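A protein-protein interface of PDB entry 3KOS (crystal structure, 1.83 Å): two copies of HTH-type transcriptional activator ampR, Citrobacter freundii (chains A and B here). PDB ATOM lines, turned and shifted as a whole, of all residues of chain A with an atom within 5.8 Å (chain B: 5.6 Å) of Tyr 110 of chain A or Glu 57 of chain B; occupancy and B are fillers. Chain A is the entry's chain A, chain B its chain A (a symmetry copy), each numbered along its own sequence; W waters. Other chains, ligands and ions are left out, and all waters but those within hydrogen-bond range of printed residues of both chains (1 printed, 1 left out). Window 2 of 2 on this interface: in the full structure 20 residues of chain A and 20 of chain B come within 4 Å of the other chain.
No position is printed for both chains. Of the 7 pairs that touch across the chains among the printed residues, none has its exchanged pair printed and touching as well.
The backbone carbonyl oxygen (O) of Glu 57 of chain B sits at hydrogen-bond distance from the side-chain amino group (NZ) of Lys 15 of chain B (2.8 Å). NH1 of Arg 51 of chain A sits at hydrogen-bond distance from O of Asp 137 of chain A (2.8 Å). A ring nitrogen (NE2) of His 48 of chain B lies within hydrogen-bond range of the backbone carbonyl oxygen (O) of Gly 17 of chain B (3.0 Å). The backbone carbonyl oxygen of Arg 108 of chain A is in hydrogen-bond range of the backbone NH of Phe 136 of chain A.
Among the printed residues, pairs that only touch across the chains: Val 135 of chain A with Ser 46 of chain B, Asp 137 of chain A with His 48 of chain B, Phe 136 of chain A with Thr 47 of chain B and Tyr 110 of chain A with Glu 57 of chain B.
Water W1 lies within hydrogen-bond range of the side-chain carboxylate of Glu 57 of chain B, the side-chain hydroxyl of Tyr 110 of chain A and the side-chain hydroxyl of Ser 46 of chain B.
Of the 10 printed residues of chain A, 4 touch a printed residue of chain B. Hydrophobic or aromatic side chains of chain A that line the printed part of chain B: Tyr 110, Val 135 and Phe 136. Among the printed residues, 7 pairs touch across the chains.
Tyr 110 of chain A touches two residues of chain B. Of the printed residues of chain B, Val 135 of chain A touches Ser 46 (3.0 Å) and Thr 47 (2.9 Å). Printed residues of chain B within 4 Å of Phe 136 of chain A: Thr 47. Printed residues of chain B within 4 Å of Asp 137 of chain A: Thr 47 (2.7 Å) and His 48 (3.3 Å). Of the printed residues of chain A, Ser 46 of chain B touches Val 135. Printed residues of chain A within 4 Å of His 48 of chain B: Asp 137. The nearest residue of chain B that does not touch Tyr 110 of chain A is Ser 46 of chain B (4.1 Å). The nearest printed residue of chain A that does not touch Glu 57 of chain B is Arg 51 of chain A (6.8 Å). The nearest printed residue of chain A that does not touch Ser 46 of chain B is Tyr 110 of chain A (4.1 Å).
The side-chain carboxylate (OD1) of Asp 137 of chain A lies within hydrogen-bond range of the side-chain hydroxyl (OG1) of Thr 47 of chain B (2.7 Å). The side-chain hydroxyl (OH) of Tyr 110 of chain A sits at hydrogen-bond distance from the backbone carbonyl oxygen (O) of Thr 47 of chain B (2.8 Å). The backbone carbonyl oxygen of Val 135 of chain A lies within hydrogen-bond range of the backbone NH of Thr 47 of chain B (2.9 Å).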
ATOM      1  N   ARG A  51      -2.908  23.751   8.322  1.00  0.00           N
ATOM      2  CA  ARG A  51      -3.275  22.548   9.071  1.00  0.00           C
ATOM      3  C   ARG A  51      -1.991  21.933   9.543  1.00  0.00           C
ATOM      4  O   ARG A  51      -1.227  21.358   8.753  1.00  0.00           O
ATOM      5  CB  ARG A  51      -4.024  21.534   8.204  1.00  0.00           C
ATOM      6  CG  ARG A  51      -5.394  21.980   7.799  1.00  0.00           C
ATOM      7  CD  ARG A  51      -5.288  22.949   6.648  1.00  0.00           C
ATOM      8  NE  ARG A  51      -6.589  23.220   6.054  1.00  0.00           N
ATOM      9  CZ  ARG A  51      -6.777  24.052   5.036  1.00  0.00           C
ATOM     10  NH1 ARG A  51      -5.741  24.677   4.490  1.00  0.00           N
ATOM     11  NH2 ARG A  51      -8.000  24.261   4.567  1.00  0.00           N
ATOM     12  N   ARG A 108     -11.695  29.465  -4.000  1.00  0.00           N
ATOM     13  CA  ARG A 108     -11.810  29.767  -2.576  1.00  0.00           C
ATOM     14  C   ARG A 108     -10.980  28.810  -1.729  1.00  0.00           C
ATOM     15  O   ARG A 108     -10.459  27.814  -2.230  1.00  0.00           O
ATOM     16  CB  ARG A 108     -13.270  29.721  -2.131  1.00  0.00           C
ATOM     17  CG  ARG A 108     -13.909  28.349  -2.215  1.00  0.00           C
ATOM     18  CD  ARG A 108     -15.174  28.325  -1.371  1.00  0.00           C
ATOM     19  NE  ARG A 108     -15.949  27.101  -1.530  1.00  0.00           N
ATOM     20  CZ  ARG A 108     -15.732  25.975  -0.857  1.00  0.00           C
ATOM     21  NH1 ARG A 108     -14.744  25.889   0.017  1.00  0.00           N
ATOM     22  NH2 ARG A 108     -16.507  24.923  -1.069  1.00  0.00           N
ATOM     23  N   SER A 109     -10.838  29.135  -0.445  1.00  0.00           N
ATOM     24  CA  SER A 109     -10.157  28.253   0.493  1.00  0.00           C
ATOM     25  C   SER A 109     -11.136  27.196   0.984  1.00  0.00           C
ATOM     26  O   SER A 109     -12.273  27.130   0.519  1.00  0.00           O
ATOM     27  CB  SER A 109      -9.655  29.047   1.697  1.00  0.00           C
ATOM     28  OG  SER A 109     -10.740  29.294   2.581  1.00  0.00           O
ATOM     29  N   TYR A 110     -10.697  26.381   1.937  1.00  0.00           N
ATOM     30  CA  TYR A 110     -11.564  25.368   2.534  1.00  0.00           C
ATOM     31  C   TYR A 110     -12.728  25.944   3.343  1.00  0.00           C
ATOM     32  O   TYR A 110     -13.572  25.190   3.823  1.00  0.00           O
ATOM     33  CB  TYR A 110     -10.761  24.431   3.423  1.00  0.00           C
ATOM     34  CG  TYR A 110     -10.044  23.317   2.699  1.00  0.00           C
ATOM     35  CD1 TYR A 110      -9.266  23.571   1.576  1.00  0.00           C
ATOM     36  CD2 TYR A 110     -10.115  22.009   3.166  1.00  0.00           C
ATOM     37  CE1 TYR A 110      -8.587  22.545   0.921  1.00  0.00           C
ATOM     38  CE2 TYR A 110      -9.444  20.980   2.526  1.00  0.00           C
ATOM     39  CZ  TYR A 110      -8.681  21.255   1.405  1.00  0.00           C
ATOM     40  OH  TYR A 110      -8.010  20.230   0.774  1.00  0.00           O
ATOM     41  N   ARG A 111     -12.767  27.266   3.509  1.00  0.00           N
ATOM     42  CA  ARG A 111     -13.932  27.918   4.111  1.00  0.00           C
ATOM     43  C   ARG A 111     -15.058  28.137   3.101  1.00  0.00           C
ATOM     44  O   ARG A 111     -14.952  28.960   2.180  1.00  0.00           O
ATOM     45  CB  ARG A 111     -13.551  29.242   4.758  1.00  0.00           C
ATOM     46  CG  ARG A 111     -14.766  30.068   5.116  1.00  0.00           C
ATOM     47  CD  ARG A 111     -14.577  30.753   6.438  1.00  0.00           C
ATOM     48  NE  ARG A 111     -15.824  31.344   6.911  1.00  0.00           N
ATOM     49  CZ  ARG A 111     -15.912  32.056   8.024  1.00  0.00           C
ATOM     50  NH1 ARG A 111     -14.821  32.251   8.751  1.00  0.00           N
ATOM     51  NH2 ARG A 111     -17.076  32.572   8.404  1.00  0.00           N
ATOM     52  N   ARG A 112     -16.159  27.428   3.315  1.00  0.00           N
ATOM     53  CA  ARG A 112     -17.209  27.300   2.304  1.00  0.00           C
ATOM     54  C   ARG A 112     -17.986  28.574   1.967  1.00  0.00           C
ATOM     55  O   ARG A 112     -18.571  28.675   0.888  1.00  0.00           O
ATOM     56  CB  ARG A 112     -18.187  26.188   2.703  1.00  0.00           C
ATOM     57  N   GLU A 114     -16.881  31.950   1.994  1.00  0.00           N
ATOM     58  CA  GLU A 114     -16.134  33.175   1.690  1.00  0.00           C
ATOM     59  C   GLU A 114     -16.805  34.016   0.602  1.00  0.00           C
ATOM     60  O   GLU A 114     -16.942  35.237   0.735  1.00  0.00           O
ATOM     61  CB  GLU A 114     -14.701  32.843   1.269  1.00  0.00           C
ATOM     62  CG  GLU A 114     -13.830  32.334   2.403  1.00  0.00           C
ATOM     63  CD  GLU A 114     -12.487  31.823   1.916  1.00  0.00           C
ATOM     64  OE1 GLU A 114     -12.377  31.453   0.728  1.00  0.00           O
ATOM     65  OE2 GLU A 114     -11.544  31.784   2.728  1.00  0.00           O
ATOM     66  N   VAL A 135     -11.324  24.571  -4.863  1.00  0.00           N
ATOM     67  CA  VAL A 135     -11.037  24.774  -3.450  1.00  0.00           C
ATOM     68  C   VAL A 135      -9.552  24.577  -3.152  1.00  0.00           C
ATOM     69  O   VAL A 135      -8.967  23.587  -3.573  1.00  0.00           O
ATOM     70  CB  VAL A 135     -11.856  23.770  -2.605  1.00  0.00           C
ATOM     71  CG1 VAL A 135     -11.511  23.901  -1.129  1.00  0.00           C
ATOM     72  CG2 VAL A 135     -13.352  23.995  -2.843  1.00  0.00           C
ATOM     73  N   PHE A 136      -8.951  25.506  -2.405  1.00  0.00           N
ATOM     74  CA  PHE A 136      -7.505  25.507  -2.196  1.00  0.00           C
ATOM     75  C   PHE A 136      -7.078  25.477  -0.731  1.00  0.00           C
ATOM     76  O   PHE A 136      -7.618  26.211   0.090  1.00  0.00           O
ATOM     77  CB  PHE A 136      -6.889  26.742  -2.854  1.00  0.00           C
ATOM     78  CG  PHE A 136      -7.034  26.744  -4.334  1.00  0.00           C
ATOM     79  CD1 PHE A 136      -6.038  26.212  -5.135  1.00  0.00           C
ATOM     80  CD2 PHE A 136      -8.187  27.222  -4.927  1.00  0.00           C
ATOM     81  CE1 PHE A 136      -6.175  26.187  -6.517  1.00  0.00           C
ATOM     82  CE2 PHE A 136      -8.339  27.191  -6.313  1.00  0.00           C
ATOM     83  CZ  PHE A 136      -7.337  26.671  -7.104  1.00  0.00           C
ATOM     84  N   ASP A 137      -6.091  24.636  -0.430  1.00  0.00           N
ATOM     85  CA  ASP A 137      -5.553  24.538   0.921  1.00  0.00           C
ATOM     86  C   ASP A 137      -4.669  25.738   1.237  1.00  0.00           C
ATOM     87  O   ASP A 137      -4.482  26.098   2.402  1.00  0.00           O
ATOM     88  CB  ASP A 137      -4.748  23.248   1.088  1.00  0.00           C
ATOM     89  CG  ASP A 137      -3.503  23.207   0.201  1.00  0.00           C
ATOM     90  OD1 ASP A 137      -3.567  23.629  -0.979  1.00  0.00           O
ATOM     91  OD2 ASP A 137      -2.455  22.724   0.681  1.00  0.00           O
ATOM     92  N   LYS B  15     -15.069  13.678  -6.911  1.00  0.00           N
ATOM     93  CA  LYS B  15     -14.355  14.531  -5.964  1.00  0.00           C
ATOM     94  C   LYS B  15     -12.893  14.119  -5.904  1.00  0.00           C
ATOM     95  O   LYS B  15     -12.565  12.972  -5.587  1.00  0.00           O
ATOM     96  CB  LYS B  15     -15.001  14.457  -4.575  1.00  0.00           C
ATOM     97  CG  LYS B  15     -14.673  15.664  -3.721  1.00  0.00           C
ATOM     98  CD  LYS B  15     -15.222  15.591  -2.289  1.00  0.00           C
ATOM     99  CE  LYS B  15     -14.768  16.834  -1.512  1.00  0.00           C
ATOM    100  NZ  LYS B  15     -15.072  16.778  -0.049  1.00  0.00           N
ATOM    101  N   GLY B  17      -8.878  15.251  -4.691  1.00  0.00           N
ATOM    102  CA  GLY B  17      -7.939  16.083  -3.950  1.00  0.00           C
ATOM    103  C   GLY B  17      -6.567  15.984  -4.594  1.00  0.00           C
ATOM    104  O   GLY B  17      -5.987  14.901  -4.653  1.00  0.00           O
ATOM    105  N   SER B  46     -10.140  19.950  -5.168  1.00  0.00           N
ATOM    106  CA  SER B  46      -9.566  20.661  -4.027  1.00  0.00           C
ATOM    107  C   SER B  46      -8.078  20.359  -4.025  1.00  0.00           C
ATOM    108  O   SER B  46      -7.666  19.334  -4.556  1.00  0.00           O
ATOM    109  CB  SER B  46     -10.214  20.202  -2.720  1.00  0.00           C
ATOM    110  OG  SER B  46     -10.032  18.810  -2.529  1.00  0.00           O
ATOM    111  N   THR B  47      -7.266  21.258  -3.476  1.00  0.00           N
ATOM    112  CA  THR B  47      -5.830  21.013  -3.436  1.00  0.00           C
ATOM    113  C   THR B  47      -5.370  20.705  -2.017  1.00  0.00           C
ATOM    114  O   THR B  47      -6.024  21.075  -1.041  1.00  0.00           O
ATOM    115  CB  THR B  47      -5.005  22.208  -3.996  1.00  0.00           C
ATOM    116  OG1 THR B  47      -5.190  23.348  -3.153  1.00  0.00           O
ATOM    117  CG2 THR B  47      -5.442  22.544  -5.422  1.00  0.00           C
ATOM    118  N   HIS B  48      -4.236  20.028  -1.914  1.00  0.00           N
ATOM    119  CA  HIS B  48      -3.655  19.690  -0.622  1.00  0.00           C
ATOM    120  C   HIS B  48      -2.134  19.780  -0.727  1.00  0.00           C
ATOM    121  O   HIS B  48      -1.599  20.020  -1.816  1.00  0.00           O
ATOM    122  CB  HIS B  48      -4.114  18.294  -0.161  1.00  0.00           C
ATOM    123  CG  HIS B  48      -3.817  17.186  -1.134  1.00  0.00           C
ATOM    124  ND1 HIS B  48      -2.557  16.647  -1.288  1.00  0.00           N
ATOM    125  CD2 HIS B  48      -4.624  16.489  -1.971  1.00  0.00           C
ATOM    126  CE1 HIS B  48      -2.598  15.681  -2.188  1.00  0.00           C
ATOM    127  NE2 HIS B  48      -3.839  15.567  -2.619  1.00  0.00           N
ATOM    128  N   VAL B  52      -2.664  14.313   3.375  1.00  0.00           N
ATOM    129  CA  VAL B  52      -4.094  14.334   3.197  1.00  0.00           C
ATOM    130  C   VAL B  52      -4.680  12.997   3.620  1.00  0.00           C
ATOM    131  O   VAL B  52      -4.025  11.960   3.537  1.00  0.00           O
ATOM    132  CB  VAL B  52      -4.449  14.632   1.727  1.00  0.00           C
ATOM    133  CG1 VAL B  52      -3.913  13.542   0.817  1.00  0.00           C
ATOM    134  CG2 VAL B  52      -5.948  14.816   1.558  1.00  0.00           C
ATOM    135  N   ASP B  53      -5.910  13.048   4.101  1.00  0.00           N
ATOM    136  CA  ASP B  53      -6.633  11.869   4.536  1.00  0.00           C
ATOM    137  C   ASP B  53      -7.883  11.781   3.681  1.00  0.00           C
ATOM    138  O   ASP B  53      -8.876  12.465   3.951  1.00  0.00           O
ATOM    139  CB  ASP B  53      -7.018  12.015   6.006  1.00  0.00           C
ATOM    140  CG  ASP B  53      -7.659  10.763   6.572  1.00  0.00           C
ATOM    141  OD1 ASP B  53      -8.338  10.035   5.815  1.00  0.00           O
ATOM    142  OD2 ASP B  53      -7.490  10.518   7.786  1.00  0.00           O
ATOM    143  N   PRO B  54      -7.836  10.951   2.628  1.00  0.00           N
ATOM    144  CA  PRO B  54      -8.952  10.867   1.678  1.00  0.00           C
ATOM    145  C   PRO B  54     -10.275  10.536   2.354  1.00  0.00           C
ATOM    146  O   PRO B  54     -11.306  11.128   2.025  1.00  0.00           O
ATOM    147  CB  PRO B  54      -8.547   9.718   0.748  1.00  0.00           C
ATOM    148  CG  PRO B  54      -7.111   9.523   0.937  1.00  0.00           C
ATOM    149  CD  PRO B  54      -6.731  10.039   2.292  1.00  0.00           C
ATOM    150  N   ALA B  55     -10.253   9.592   3.292  1.00  0.00           N
ATOM    151  CA  ALA B  55     -11.491   9.192   3.953  1.00  0.00           C
ATOM    152  C   ALA B  55     -12.098  10.385   4.681  1.00  0.00           C
ATOM    153  O   ALA B  55     -13.285  10.659   4.556  1.00  0.00           O
ATOM    154  CB  ALA B  55     -11.241   8.037   4.920  1.00  0.00           C
ATOM    155  N   ALA B  56     -11.260  11.093   5.437  1.00  0.00           N
ATOM    156  CA  ALA B  56     -11.694  12.259   6.193  1.00  0.00           C
ATOM    157  C   ALA B  56     -12.279  13.338   5.287  1.00  0.00           C
ATOM    158  O   ALA B  56     -13.249  13.997   5.648  1.00  0.00           O
ATOM    159  CB  ALA B  56     -10.534  12.823   7.016  1.00  0.00           C
ATOM    160  N   GLU B  57     -11.693  13.515   4.106  1.00  0.00           N
ATOM    161  CA  GLU B  57     -12.164  14.550   3.191  1.00  0.00           C
ATOM    162  C   GLU B  57     -13.232  14.049   2.229  1.00  0.00           C
ATOM    163  O   GLU B  57     -13.750  14.816   1.426  1.00  0.00           O
ATOM    164  CB  GLU B  57     -10.998  15.165   2.412  1.00  0.00           C
ATOM    165  CG  GLU B  57     -10.049  15.959   3.286  1.00  0.00           C
ATOM    166  CD  GLU B  57      -9.084  16.827   2.483  1.00  0.00           C
ATOM    167  OE1 GLU B  57      -9.294  17.006   1.257  1.00  0.00           O
ATOM    168  OE2 GLU B  57      -8.114  17.335   3.085  1.00  0.00           O
ATOM    169  N   GLY B  58     -13.574  12.767   2.328  1.00  0.00           N
ATOM    170  CA  GLY B  58     -14.572  12.188   1.447  1.00  0.00           C
ATOM    171  C   GLY B  58     -14.183  12.271  -0.019  1.00  0.00           C
ATOM    172  O   GLY B  58     -15.027  12.497  -0.890  1.00  0.00           O
ATOM    173  N   LEU B  59     -12.904  12.062  -0.301  1.00  0.00           N
ATOM    174  CA  LEU B  59     -12.418  12.090  -1.676  1.00  0.00           C
ATOM    175  C   LEU B  59     -12.705  10.794  -2.426  1.00  0.00           C
ATOM    176  O   LEU B  59     -12.715   9.715  -1.834  1.00  0.00           O
ATOM    177  CB  LEU B  59     -10.912  12.336  -1.696  1.00  0.00           C
ATOM    178  CG  LEU B  59     -10.417  13.614  -1.015  1.00  0.00           C
ATOM    179  CD1 LEU B  59      -8.896  13.664  -1.081  1.00  0.00           C
ATOM    180  CD2 LEU B  59     -11.039  14.853  -1.654  1.00  0.00           C
HETATM  181  O   HOH W   1      -7.691  17.905  -0.895  1.00  0.00           O
